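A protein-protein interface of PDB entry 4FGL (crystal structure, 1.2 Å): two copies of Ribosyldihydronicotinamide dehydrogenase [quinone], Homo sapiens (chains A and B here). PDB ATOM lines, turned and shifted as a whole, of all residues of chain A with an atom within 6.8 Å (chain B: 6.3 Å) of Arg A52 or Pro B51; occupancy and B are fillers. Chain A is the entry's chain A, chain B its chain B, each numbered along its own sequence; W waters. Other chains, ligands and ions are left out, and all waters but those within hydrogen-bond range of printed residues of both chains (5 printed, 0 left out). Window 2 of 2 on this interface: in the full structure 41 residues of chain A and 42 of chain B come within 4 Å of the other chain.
Arg A52 touches just these residues of chain B: Asn B48 (3.0 Å), Phe B49 (2.9 Å), Glu B50 (3.5 Å), Pro B51 (3.7 Å) and Ile B114 (3.95 Å).
Of chain A, only Pro A51 (3.8 Å), Arg A52 (3.7 Å) and Ala A113 (3.4 Å) come within 4 Å of Pro B51.
Of the printed residues of chain B, Tyr A45 touches Ala B53.
Of the printed residues of chain A, Gly B117 touches Ala A113 (3.4 Å).
Printed residues of chain A within 4 Å of Ala B53: Tyr A45.
Of the printed residues of chain A, Ala B113 touches Pro A51, Ala A113, Gly A117 and Asp A120.
The nearest residue of chain B that does not touch Arg A52 is Arg B52 (4.2 Å).
Of the 16 printed residues of chain A, 11 touch a printed residue of chain B.
Printed residues of chain A that touch a printed residue of chain B: Tyr A45, Phe A49, Glu A50, Pro A51, Arg A52, Ala A53, Tyr A70, Pro A112, Ala A113, Gly A117 and Asp A120.
Along chain A the printed residues that touch a printed residue of chain B span positions 45 to 120.
Of the 17 printed residues of chain B, 13 touch a printed residue of chain A.
Hydrophobic or aromatic side chains of chain B within 4 Å of the printed part of chain A: Tyr B45, Pro B51, Ala B113 and Ile B114.
Along chain B the printed residues that touch a printed residue of chain A span positions 15 to 120.
Among the printed residues, 22 pairs touch across the chains.
Among the printed residues, no Asp or Glu carboxylate lies within 4 Å of a Lys or Arg side-chain nitrogen of the other chain.
Among the printed residues, pairs that only touch across the chains: Tyr A45 with Ala B53, Ala A53 with Tyr B45, Gly A117 with Ala B113, Ala A113 with Gly B117, Ala A113 with Pro B51, Pro A51 with Ala B113, Glu A50 with Arg B52, Arg A52 with Glu B50, Ala A113 with Ala B113, Pro A51 with Arg B52, Arg A52 with Pro B51, Pro A112 with Asp B120, Pro A51 with Pro B51, Ala A113 with Lys B116, Tyr A70 with Gln B15 and Arg A52 with Ile B114.
Tyr A45 touches Ala B53, and with the chains exchanged Ala A53 touches Tyr B45.
Phe A49 touches Arg B52, and with the chains exchanged Arg A52 touches Phe B49.
Glu A50 touches Arg B52, and with the chains exchanged Arg A52 touches Glu B50.
Arg A52 touches Ile B114, but with the chains exchanged Ile A114 does not touch Arg B52 (4.1 Å).
Of the 22 pairs that touch across the chains among the printed residues, 16 have their exchanged pair printed and touching as well.
The guanidinium group (NE) of Arg B52 lies within hydrogen-bond range of the backbone carbonyl oxygen (O) of Phe A49, at 2.9 Å.
O of Asn B48 sits at hydrogen-bond distance from NH2 of Arg A52 (3.0 Å).
The guanidinium group (NE) of Arg A52 lies within hydrogen-bond range of the backbone carbonyl oxygen (O) of Phe B49 (2.9 Å).
The side-chain amide nitrogen of Gln B15 sits at hydrogen-bond distance from the backbone carbonyl oxygen of Ala A53, at 2.8 Å.
The backbone NH of Ala A113 sits at hydrogen-bond distance from the side-chain carboxylate of Asp B120, at 2.9 Å.
OD2 of Asp A120 lies within hydrogen-bond range of N of Ala B113, 2.9 Å away.
Water W2 lies within hydrogen-bond range of OE1 of Glu A50 (2.7 Å), NH2 of Arg B52 (2.8 Å) and NH1 of Arg A52 (3.0 Å).
Water W4 lies within hydrogen-bond range of OE1 of Glu B50 (2.8 Å), NH2 of Arg A52 (2.9 Å) and NH1 of Arg B52 (3.0 Å).
Water W3 lies within hydrogen-bond range of OH of Tyr B45 (2.8 Å), N of Ile B114 (3.0 Å) and N of Ala A53 (3.4 Å).
Water W1 lies within hydrogen-bond range of the backbone NH (N) of Tyr A70 (2.9 Å) and the side-chain amide oxygen (OE1) of Gln B15 (2.9 Å).
Water W5 lies within hydrogen-bond range of the side-chain hydroxyl of Tyr A45, the backbone NH of Ile A114 and the backbone NH of Ala B53.
OE2 of Glu A50 is in salt-bridge range of NH1 of Arg A52, at 2.9 Å.
NE of Arg A121 sits close to O of Arg A52 (3.4 Å).
OD2 of Asp A57 lies within hydrogen-bond range of OH of Tyr A70 (2.6 Å).
The side-chain amide nitrogen of Gln B15 lies within hydrogen-bond range of the side-chain hydroxyl of Tyr B45 (3.3 Å).
O of Leu B44 lies within hydrogen-bond range of N of Phe B49.
The side-chain carboxylate (OE2) of Glu B50 is in salt-bridge range of the guanidinium group (NH1) of Arg B52 (3.0 Å).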
ATOM      1  N   TYR A  45      15.737  38.282  -8.808  1.00  0.00           N
ATOM      2  CA  TYR A  45      16.529  38.640  -7.633  1.00  0.00           C
ATOM      3  C   TYR A  45      16.179  40.034  -7.127  1.00  0.00           C
ATOM      4  O   TYR A  45      16.119  40.244  -5.920  1.00  0.00           O
ATOM      5  CB  TYR A  45      18.016  38.554  -7.889  1.00  0.00           C
ATOM      6  CG  TYR A  45      18.564  37.142  -8.038  1.00  0.00           C
ATOM      7  CD1 TYR A  45      18.820  36.324  -6.929  1.00  0.00           C
ATOM      8  CD2 TYR A  45      18.865  36.629  -9.287  1.00  0.00           C
ATOM      9  CE1 TYR A  45      19.355  35.040  -7.096  1.00  0.00           C
ATOM     10  CE2 TYR A  45      19.388  35.363  -9.452  1.00  0.00           C
ATOM     11  CZ  TYR A  45      19.636  34.574  -8.350  1.00  0.00           C
ATOM     12  OH  TYR A  45      20.190  33.334  -8.509  1.00  0.00           O
ATOM     13  N   PHE A  49      12.259  37.354  -5.181  1.00  0.00           N
ATOM     14  CA  PHE A  49      11.187  36.421  -5.467  1.00  0.00           C
ATOM     15  C   PHE A  49      11.285  35.174  -4.599  1.00  0.00           C
ATOM     16  O   PHE A  49      12.357  34.548  -4.471  1.00  0.00           O
ATOM     17  CB  PHE A  49      11.246  36.013  -6.938  1.00  0.00           C
ATOM     18  CG  PHE A  49      10.034  35.265  -7.394  1.00  0.00           C
ATOM     19  CD1 PHE A  49       8.889  35.944  -7.706  1.00  0.00           C
ATOM     20  CD2 PHE A  49      10.022  33.885  -7.455  1.00  0.00           C
ATOM     21  CE1 PHE A  49       7.750  35.265  -8.090  1.00  0.00           C
ATOM     22  CE2 PHE A  49       8.899  33.215  -7.843  1.00  0.00           C
ATOM     23  CZ  PHE A  49       7.766  33.891  -8.145  1.00  0.00           C
ATOM     24  N   GLU A  50      10.164  34.794  -4.005  1.00  0.00           N
ATOM     25  CA  GLU A  50      10.071  33.635  -3.129  1.00  0.00           C
ATOM     26  C   GLU A  50      10.167  32.348  -3.926  1.00  0.00           C
ATOM     27  O   GLU A  50       9.319  32.079  -4.775  1.00  0.00           O
ATOM     28  CB  GLU A  50       8.726  33.662  -2.402  1.00  0.00           C
ATOM     29  CG  GLU A  50       8.458  32.408  -1.580  1.00  0.00           C
ATOM     30  CD  GLU A  50       9.439  32.205  -0.464  1.00  0.00           C
ATOM     31  OE1 GLU A  50       9.402  33.001   0.498  1.00  0.00           O
ATOM     32  OE2 GLU A  50      10.246  31.258  -0.520  1.00  0.00           O
ATOM     33  N   PRO A  51      11.167  31.497  -3.616  1.00  0.00           N
ATOM     34  CA  PRO A  51      11.246  30.259  -4.402  1.00  0.00           C
ATOM     35  C   PRO A  51      10.517  29.073  -3.776  1.00  0.00           C
ATOM     36  O   PRO A  51      10.271  28.093  -4.467  1.00  0.00           O
ATOM     37  CB  PRO A  51      12.760  29.946  -4.457  1.00  0.00           C
ATOM     38  CG  PRO A  51      13.453  31.154  -3.867  1.00  0.00           C
ATOM     39  CD  PRO A  51      12.447  31.768  -2.946  1.00  0.00           C
ATOM     40  N   ARG A  52      10.212  29.131  -2.488  1.00  0.00           N
ATOM     41  CA  ARG A  52       9.720  27.949  -1.783  1.00  0.00           C
ATOM     42  C   ARG A  52       8.228  27.763  -2.011  1.00  0.00           C
ATOM     43  O   ARG A  52       7.459  28.737  -1.921  1.00  0.00           O
ATOM     44  CB  ARG A  52       9.962  28.080  -0.278  1.00  0.00           C
ATOM     45  CG  ARG A  52      11.417  28.316   0.148  1.00  0.00           C
ATOM     46  CD  ARG A  52      11.407  28.630   1.624  1.00  0.00           C
ATOM     47  NE  ARG A  52      12.622  29.204   2.198  1.00  0.00           N
ATOM     48  CZ  ARG A  52      12.910  30.497   2.283  1.00  0.00           C
ATOM     49  NH1 ARG A  52      12.146  31.410   1.714  1.00  0.00           N
ATOM     50  NH2 ARG A  52      13.992  30.871   2.923  1.00  0.00           N
ATOM     51  N   ALA A  53       7.804  26.532  -2.278  1.00  0.00           N
ATOM     52  CA  ALA A  53       6.396  26.157  -2.397  1.00  0.00           C
ATOM     53  C   ALA A  53       5.853  25.885  -1.004  1.00  0.00           C
ATOM     54  O   ALA A  53       6.122  24.834  -0.419  1.00  0.00           O
ATOM     55  CB  ALA A  53       6.265  24.910  -3.291  1.00  0.00           C
ATOM     56  N   THR A  54       5.129  26.846  -0.430  1.00  0.00           N
ATOM     57  CA  THR A  54       4.609  26.682   0.929  1.00  0.00           C
ATOM     58  C   THR A  54       3.148  27.103   1.013  1.00  0.00           C
ATOM     59  O   THR A  54       2.586  27.689   0.076  1.00  0.00           O
ATOM     60  CB  THR A  54       5.391  27.506   1.986  1.00  0.00           C
ATOM     61  OG1 THR A  54       4.978  28.871   1.938  1.00  0.00           O
ATOM     62  CG2 THR A  54       6.910  27.366   1.820  1.00  0.00           C
ATOM     63  N   ASP A  55       2.565  26.851   2.189  1.00  0.00           N
ATOM     64  CA  ASP A  55       1.179  27.176   2.437  1.00  0.00           C
ATOM     65  C   ASP A  55       0.924  28.674   2.417  1.00  0.00           C
ATOM     66  O   ASP A  55      -0.233  29.096   2.304  1.00  0.00           O
ATOM     67  CB  ASP A  55       0.671  26.519   3.741  1.00  0.00           C
ATOM     68  CG  ASP A  55       1.358  27.023   5.011  1.00  0.00           C
ATOM     69  OD1 ASP A  55       2.409  27.677   4.983  1.00  0.00           O
ATOM     70  OD2 ASP A  55       0.809  26.717   6.097  1.00  0.00           O
ATOM     71  N   ASP A  57       1.516  30.429   0.011  1.00  0.00           N
ATOM     72  CA  ASP A  57       1.140  30.719  -1.368  1.00  0.00           C
ATOM     73  C   ASP A  57      -0.369  30.795  -1.579  1.00  0.00           C
ATOM     74  O   ASP A  57      -0.840  31.227  -2.628  1.00  0.00           O
ATOM     75  CB  ASP A  57       1.774  29.691  -2.305  1.00  0.00           C
ATOM     76  CG  ASP A  57       3.285  29.812  -2.342  1.00  0.00           C
ATOM     77  OD1 ASP A  57       3.799  30.808  -1.783  1.00  0.00           O
ATOM     78  OD2 ASP A  57       3.922  28.935  -2.944  1.00  0.00           O
ATOM     79  N   TYR A  70       0.294  20.767  -1.369  1.00  0.00           N
ATOM     80  CA  TYR A  70       0.583  21.975  -2.148  1.00  0.00           C
ATOM     81  C   TYR A  70      -0.180  21.977  -3.483  1.00  0.00           C
ATOM     82  O   TYR A  70      -0.792  22.986  -3.858  1.00  0.00           O
ATOM     83  CB  TYR A  70       2.098  22.131  -2.378  1.00  0.00           C
ATOM     84  CG  TYR A  70       2.439  23.459  -3.005  1.00  0.00           C
ATOM     85  CD1 TYR A  70       2.510  24.600  -2.246  1.00  0.00           C
ATOM     86  CD2 TYR A  70       2.615  23.574  -4.382  1.00  0.00           C
ATOM     87  CE1 TYR A  70       2.780  25.817  -2.816  1.00  0.00           C
ATOM     88  CE2 TYR A  70       2.894  24.784  -4.975  1.00  0.00           C
ATOM     89  CZ  TYR A  70       2.965  25.911  -4.188  1.00  0.00           C
ATOM     90  OH  TYR A  70       3.234  27.143  -4.740  1.00  0.00           O
ATOM     91  N   PRO A 112      18.840  28.437 -11.983  1.00  0.00           N
ATOM     92  CA  PRO A 112      19.028  28.824 -10.578  1.00  0.00           C
ATOM     93  C   PRO A 112      17.773  28.582  -9.771  1.00  0.00           C
ATOM     94  O   PRO A 112      16.659  28.730 -10.283  1.00  0.00           O
ATOM     95  CB  PRO A 112      19.343  30.332 -10.666  1.00  0.00           C
ATOM     96  CG  PRO A 112      19.946  30.501 -12.066  1.00  0.00           C
ATOM     97  CD  PRO A 112      19.145  29.547 -12.904  1.00  0.00           C
ATOM     98  N   ALA A 113      17.932  28.284  -8.488  1.00  0.00           N
ATOM     99  CA  ALA A 113      16.785  27.968  -7.654  1.00  0.00           C
ATOM    100  C   ALA A 113      15.716  29.048  -7.654  1.00  0.00           C
ATOM    101  O   ALA A 113      14.536  28.709  -7.568  1.00  0.00           O
ATOM    102  CB  ALA A 113      17.213  27.650  -6.207  1.00  0.00           C
ATOM    103  N   ILE A 114      16.082  30.318  -7.727  1.00  0.00           N
ATOM    104  CA  ILE A 114      15.042  31.347  -7.689  1.00  0.00           C
ATOM    105  C   ILE A 114      14.104  31.230  -8.898  1.00  0.00           C
ATOM    106  O   ILE A 114      12.890  31.449  -8.799  1.00  0.00           O
ATOM    107  CB  ILE A 114      15.670  32.754  -7.553  1.00  0.00           C
ATOM    108  CG1 ILE A 114      14.620  33.766  -7.118  1.00  0.00           C
ATOM    109  CG2 ILE A 114      16.386  33.210  -8.819  1.00  0.00           C
ATOM    110  CD1 ILE A 114      15.197  35.137  -6.766  1.00  0.00           C
ATOM    111  N   GLY A 117      11.927  28.161  -8.586  1.00  0.00           N
ATOM    112  CA  GLY A 117      10.791  28.492  -7.743  1.00  0.00           C
ATOM    113  C   GLY A 117       9.692  29.253  -8.482  1.00  0.00           C
ATOM    114  O   GLY A 117       8.510  29.020  -8.227  1.00  0.00           O
ATOM    115  N   ASP A 120       7.924  26.460 -10.279  1.00  0.00           N
ATOM    116  CA  ASP A 120       7.162  25.630  -9.373  1.00  0.00           C
ATOM    117  C   ASP A 120       5.886  26.331  -8.923  1.00  0.00           C
ATOM    118  O   ASP A 120       4.847  25.684  -8.775  1.00  0.00           O
ATOM    119  CB  ASP A 120       7.960  25.290  -8.103  1.00  0.00           C
ATOM    120  CG  ASP A 120       9.191  24.432  -8.338  1.00  0.00           C
ATOM    121  OD1 ASP A 120       9.339  23.815  -9.410  1.00  0.00           O
ATOM    122  OD2 ASP A 120      10.010  24.338  -7.377  1.00  0.00           O
ATOM    123  N   ARG A 121       5.988  27.628  -8.631  1.00  0.00           N
ATOM    124  CA  ARG A 121       4.910  28.365  -7.982  1.00  0.00           C
ATOM    125  C   ARG A 121       3.959  29.042  -8.955  1.00  0.00           C
ATOM    126  O   ARG A 121       2.762  29.173  -8.680  1.00  0.00           O
ATOM    127  CB  ARG A 121       5.492  29.417  -7.027  1.00  0.00           C
ATOM    128  CG  ARG A 121       6.274  28.815  -5.854  1.00  0.00           C
ATOM    129  CD  ARG A 121       6.988  29.893  -5.015  1.00  0.00           C
ATOM    130  NE  ARG A 121       6.038  30.704  -4.256  1.00  0.00           N
ATOM    131  CZ  ARG A 121       5.833  32.018  -4.391  1.00  0.00           C
ATOM    132  NH1 ARG A 121       6.545  32.753  -5.239  1.00  0.00           N
ATOM    133  NH2 ARG A 121       4.905  32.592  -3.647  1.00  0.00           N
ATOM    134  N   GLN B  15       6.740  19.507   2.376  1.00  0.00           N
ATOM    135  CA  GLN B  15       6.097  20.384   3.350  1.00  0.00           C
ATOM    136  C   GLN B  15       5.303  19.664   4.443  1.00  0.00           C
ATOM    137  O   GLN B  15       5.022  20.256   5.479  1.00  0.00           O
ATOM    138  CB  GLN B  15       5.119  21.329   2.646  1.00  0.00           C
ATOM    139  CG  GLN B  15       5.697  22.104   1.457  1.00  0.00           C
ATOM    140  CD  GLN B  15       5.533  21.387   0.143  1.00  0.00           C
ATOM    141  OE1 GLN B  15       5.232  20.188   0.107  1.00  0.00           O
ATOM    142  NE2 GLN B  15       5.724  22.113  -0.957  1.00  0.00           N
ATOM    143  N   LEU B  44      14.331  20.626   4.862  1.00  0.00           N
ATOM    144  CA  LEU B  44      14.535  21.966   4.312  1.00  0.00           C
ATOM    145  C   LEU B  44      13.369  22.905   4.565  1.00  0.00           C
ATOM    146  O   LEU B  44      13.574  24.055   4.920  1.00  0.00           O
ATOM    147  CB  LEU B  44      14.849  21.887   2.816  1.00  0.00           C
ATOM    148  CG  LEU B  44      16.095  21.080   2.457  1.00  0.00           C
ATOM    149  CD1 LEU B  44      16.299  21.186   0.951  1.00  0.00           C
ATOM    150  CD2 LEU B  44      17.319  21.555   3.240  1.00  0.00           C
ATOM    151  N   TYR B  45      12.133  22.440   4.403  1.00  0.00           N
ATOM    152  CA  TYR B  45      11.005  23.351   4.638  1.00  0.00           C
ATOM    153  C   TYR B  45      10.897  23.706   6.116  1.00  0.00           C
ATOM    154  O   TYR B  45      10.635  24.861   6.453  1.00  0.00           O
ATOM    155  CB  TYR B  45       9.684  22.795   4.134  1.00  0.00           C
ATOM    156  CG  TYR B  45       9.535  22.723   2.636  1.00  0.00           C
ATOM    157  CD1 TYR B  45       9.209  23.846   1.876  1.00  0.00           C
ATOM    158  CD2 TYR B  45       9.677  21.525   1.980  1.00  0.00           C
ATOM    159  CE1 TYR B  45       9.040  23.742   0.519  1.00  0.00           C
ATOM    160  CE2 TYR B  45       9.511  21.426   0.618  1.00  0.00           C
ATOM    161  CZ  TYR B  45       9.182  22.549  -0.103  1.00  0.00           C
ATOM    162  OH  TYR B  45       9.000  22.457  -1.465  1.00  0.00           O
ATOM    163  N   ASN B  48      13.154  26.368   6.971  1.00  0.00           N
ATOM    164  CA  ASN B  48      12.981  27.549   6.140  1.00  0.00           C
ATOM    165  C   ASN B  48      14.233  27.825   5.320  1.00  0.00           C
ATOM    166  O   ASN B  48      14.671  28.965   5.177  1.00  0.00           O
ATOM    167  CB  ASN B  48      12.611  28.776   6.970  1.00  0.00           C
ATOM    168  CG  ASN B  48      12.160  29.950   6.107  1.00  0.00           C
ATOM    169  OD1 ASN B  48      11.507  29.757   5.081  1.00  0.00           O
ATOM    170  ND2 ASN B  48      12.523  31.168   6.511  1.00  0.00           N
ATOM    171  N   PHE B  49      14.781  26.775   4.736  1.00  0.00           N
ATOM    172  CA  PHE B  49      16.091  26.881   4.105  1.00  0.00           C
ATOM    173  C   PHE B  49      16.097  27.909   2.983  1.00  0.00           C
ATOM    174  O   PHE B  49      15.195  27.899   2.128  1.00  0.00           O
ATOM    175  CB  PHE B  49      16.522  25.517   3.547  1.00  0.00           C
ATOM    176  CG  PHE B  49      17.949  25.495   3.117  1.00  0.00           C
ATOM    177  CD1 PHE B  49      18.958  25.353   4.036  1.00  0.00           C
ATOM    178  CD2 PHE B  49      18.298  25.690   1.793  1.00  0.00           C
ATOM    179  CE1 PHE B  49      20.288  25.366   3.631  1.00  0.00           C
ATOM    180  CE2 PHE B  49      19.628  25.704   1.416  1.00  0.00           C
ATOM    181  CZ  PHE B  49      20.600  25.551   2.325  1.00  0.00           C
ATOM    182  N   GLU B  50      17.081  28.803   2.979  1.00  0.00           N
ATOM    183  CA  GLU B  50      17.177  29.850   1.968  1.00  0.00           C
ATOM    184  C   GLU B  50      17.598  29.281   0.618  1.00  0.00           C
ATOM    185  O   GLU B  50      18.686  28.695   0.514  1.00  0.00           O
ATOM    186  CB  GLU B  50      18.228  30.871   2.406  1.00  0.00           C
ATOM    187  CG  GLU B  50      18.547  31.910   1.360  1.00  0.00           C
ATOM    188  CD  GLU B  50      17.359  32.753   1.013  1.00  0.00           C
ATOM    189  OE1 GLU B  50      16.930  33.529   1.907  1.00  0.00           O
ATOM    190  OE2 GLU B  50      16.848  32.665  -0.132  1.00  0.00           O
ATOM    191  N   PRO B  51      16.787  29.454  -0.434  1.00  0.00           N
ATOM    192  CA  PRO B  51      17.207  28.845  -1.712  1.00  0.00           C
ATOM    193  C   PRO B  51      17.961  29.798  -2.618  1.00  0.00           C
ATOM    194  O   PRO B  51      18.552  29.336  -3.579  1.00  0.00           O
ATOM    195  CB  PRO B  51      15.879  28.477  -2.385  1.00  0.00           C
ATOM    196  CG  PRO B  51      14.831  28.656  -1.321  1.00  0.00           C
ATOM    197  CD  PRO B  51      15.351  29.749  -0.454  1.00  0.00           C
ATOM    198  N   ARG B  52      17.874  31.097  -2.379  1.00  0.00           N
ATOM    199  CA  ARG B  52      18.405  32.086  -3.321  1.00  0.00           C
ATOM    200  C   ARG B  52      19.912  32.236  -3.176  1.00  0.00           C
ATOM    201  O   ARG B  52      20.425  32.370  -2.066  1.00  0.00           O
ATOM    202  CB  ARG B  52      17.763  33.452  -3.071  1.00  0.00           C
ATOM    203  CG  ARG B  52      16.224  33.496  -3.162  1.00  0.00           C
ATOM    204  CD  ARG B  52      15.785  34.873  -2.723  1.00  0.00           C
ATOM    205  NE  ARG B  52      14.355  35.063  -2.477  1.00  0.00           N
ATOM    206  CZ  ARG B  52      13.758  34.885  -1.296  1.00  0.00           C
ATOM    207  NH1 ARG B  52      14.407  34.357  -0.272  1.00  0.00           N
ATOM    208  NH2 ARG B  52      12.478  35.174  -1.165  1.00  0.00           N
ATOM    209  N   ALA B  53      20.609  32.266  -4.312  1.00  0.00           N
ATOM    210  CA  ALA B  53      22.052  32.507  -4.340  1.00  0.00           C
ATOM    211  C   ALA B  53      22.271  34.008  -4.364  1.00  0.00           C
ATOM    212  O   ALA B  53      22.049  34.631  -5.407  1.00  0.00           O
ATOM    213  CB  ALA B  53      22.643  31.882  -5.594  1.00  0.00           C
ATOM    214  N   ALA B 113      12.332  23.656  -5.760  1.00  0.00           N
ATOM    215  CA  ALA B 113      13.262  24.777  -5.714  1.00  0.00           C
ATOM    216  C   ALA B 113      13.999  24.876  -4.388  1.00  0.00           C
ATOM    217  O   ALA B 113      15.162  25.288  -4.386  1.00  0.00           O
ATOM    218  CB  ALA B 113      12.541  26.093  -6.013  1.00  0.00           C
ATOM    219  N   ILE B 114      13.375  24.547  -3.257  1.00  0.00           N
ATOM    220  CA  ILE B 114      14.106  24.656  -1.993  1.00  0.00           C
ATOM    221  C   ILE B 114      15.333  23.725  -1.964  1.00  0.00           C
ATOM    222  O   ILE B 114      16.403  24.084  -1.456  1.00  0.00           O
ATOM    223  CB  ILE B 114      13.150  24.437  -0.777  1.00  0.00           C
ATOM    224  CG1 ILE B 114      13.793  24.999   0.489  1.00  0.00           C
ATOM    225  CG2 ILE B 114      12.715  23.001  -0.652  1.00  0.00           C
ATOM    226  CD1 ILE B 114      12.862  24.954   1.693  1.00  0.00           C
ATOM    227  N   LEU B 115      15.181  22.540  -2.550  1.00  0.00           N
ATOM    228  CA  LEU B 115      16.269  21.578  -2.677  1.00  0.00           C
ATOM    229  C   LEU B 115      17.254  22.000  -3.765  1.00  0.00           C
ATOM    230  O   LEU B 115      18.469  21.860  -3.609  1.00  0.00           O
ATOM    231  CB  LEU B 115      15.693  20.173  -2.916  1.00  0.00           C
ATOM    232  CG  LEU B 115      16.723  19.074  -3.203  1.00  0.00           C
ATOM    233  CD1 LEU B 115      17.812  19.012  -2.130  1.00  0.00           C
ATOM    234  CD2 LEU B 115      16.019  17.747  -3.275  1.00  0.00           C
ATOM    235  N   LYS B 116      16.757  22.565  -4.863  1.00  0.00           N
ATOM    236  CA  LYS B 116      17.661  23.151  -5.847  1.00  0.00           C
ATOM    237  C   LYS B 116      18.565  24.206  -5.194  1.00  0.00           C
ATOM    238  O   LYS B 116      19.748  24.291  -5.479  1.00  0.00           O
ATOM    239  CB  LYS B 116      16.902  23.759  -7.026  1.00  0.00           C
ATOM    240  CG  LYS B 116      17.795  24.243  -8.164  1.00  0.00           C
ATOM    241  CD  LYS B 116      18.751  23.169  -8.627  1.00  0.00           C
ATOM    242  CE  LYS B 116      19.366  23.420  -9.999  1.00  0.00           C
ATOM    243  NZ  LYS B 116      20.109  24.705 -10.042  1.00  0.00           N
ATOM    244  N   GLY B 117      18.006  24.993  -4.288  1.00  0.00           N
ATOM    245  CA  GLY B 117      18.779  26.000  -3.604  1.00  0.00           C
ATOM    246  C   GLY B 117      19.846  25.428  -2.684  1.00  0.00           C
ATOM    247  O   GLY B 117      20.932  25.994  -2.550  1.00  0.00           O
ATOM    248  N   TRP B 118      19.519  24.326  -2.019  1.00  0.00           N
ATOM    249  CA  TRP B 118      20.516  23.596  -1.260  1.00  0.00           C
ATOM    250  C   TRP B 118      21.663  23.184  -2.186  1.00  0.00           C
ATOM    251  O   TRP B 118      22.835  23.388  -1.855  1.00  0.00           O
ATOM    252  CB  TRP B 118      19.849  22.410  -0.567  1.00  0.00           C
ATOM    253  CG  TRP B 118      20.736  21.633   0.372  1.00  0.00           C
ATOM    254  CD1 TRP B 118      20.754  21.727   1.740  1.00  0.00           C
ATOM    255  CD2 TRP B 118      21.696  20.618   0.035  1.00  0.00           C
ATOM    256  NE1 TRP B 118      21.683  20.857   2.274  1.00  0.00           N
ATOM    257  CE2 TRP B 118      22.260  20.152   1.255  1.00  0.00           C
ATOM    258  CE3 TRP B 118      22.117  20.049  -1.161  1.00  0.00           C
ATOM    259  CZ2 TRP B 118      23.257  19.175   1.286  1.00  0.00           C
ATOM    260  CZ3 TRP B 118      23.107  19.083  -1.125  1.00  0.00           C
ATOM    261  CH2 TRP B 118      23.653  18.652   0.094  1.00  0.00           C
ATOM    262  N   ASP B 120      22.583  24.513  -5.091  1.00  0.00           N
ATOM    263  CA  ASP B 120      23.242  25.707  -5.597  1.00  0.00           C
ATOM    264  C   ASP B 120      24.172  26.316  -4.532  1.00  0.00           C
ATOM    265  O   ASP B 120      25.256  26.789  -4.864  1.00  0.00           O
ATOM    266  CB  ASP B 120      22.213  26.776  -5.986  1.00  0.00           C
ATOM    267  CG  ASP B 120      21.351  26.416  -7.177  1.00  0.00           C
ATOM    268  OD1 ASP B 120      21.632  25.430  -7.876  1.00  0.00           O
ATOM    269  OD2 ASP B 120      20.376  27.191  -7.402  1.00  0.00           O
ATOM    270  N   ARG B 121      23.717  26.354  -3.278  1.00  0.00           N
ATOM    271  CA  ARG B 121      24.401  27.119  -2.237  1.00  0.00           C
ATOM    272  C   ARG B 121      25.402  26.279  -1.457  1.00  0.00           C
ATOM    273  O   ARG B 121      26.449  26.771  -1.045  1.00  0.00           O
ATOM    274  CB  ARG B 121      23.385  27.781  -1.297  1.00  0.00           C
ATOM    275  CG  ARG B 121      22.495  28.798  -2.004  1.00  0.00           C
ATOM    276  CD  ARG B 121      21.412  29.331  -1.058  1.00  0.00           C
ATOM    277  NE  ARG B 121      21.964  30.189  -0.017  1.00  0.00           N
ATOM    278  CZ  ARG B 121      21.938  29.924   1.288  1.00  0.00           C
ATOM    279  NH1 ARG B 121      21.337  28.837   1.783  1.00  0.00           N
ATOM    280  NH2 ARG B 121      22.525  30.765   2.129  1.00  0.00           N
HETATM  281  O   HOH W   1       2.389  19.449   0.050  1.00  0.00           O
HETATM  282  O   HOH W   2      11.586  34.377   1.373  1.00  0.00           O
HETATM  283  O   HOH W   3      10.432  24.451  -2.850  1.00  0.00           O
HETATM  284  O   HOH W   4      14.224  33.701   2.658  1.00  0.00           O
HETATM  285  O   HOH W   5      18.745  31.385  -7.002  1.00  0.00           O
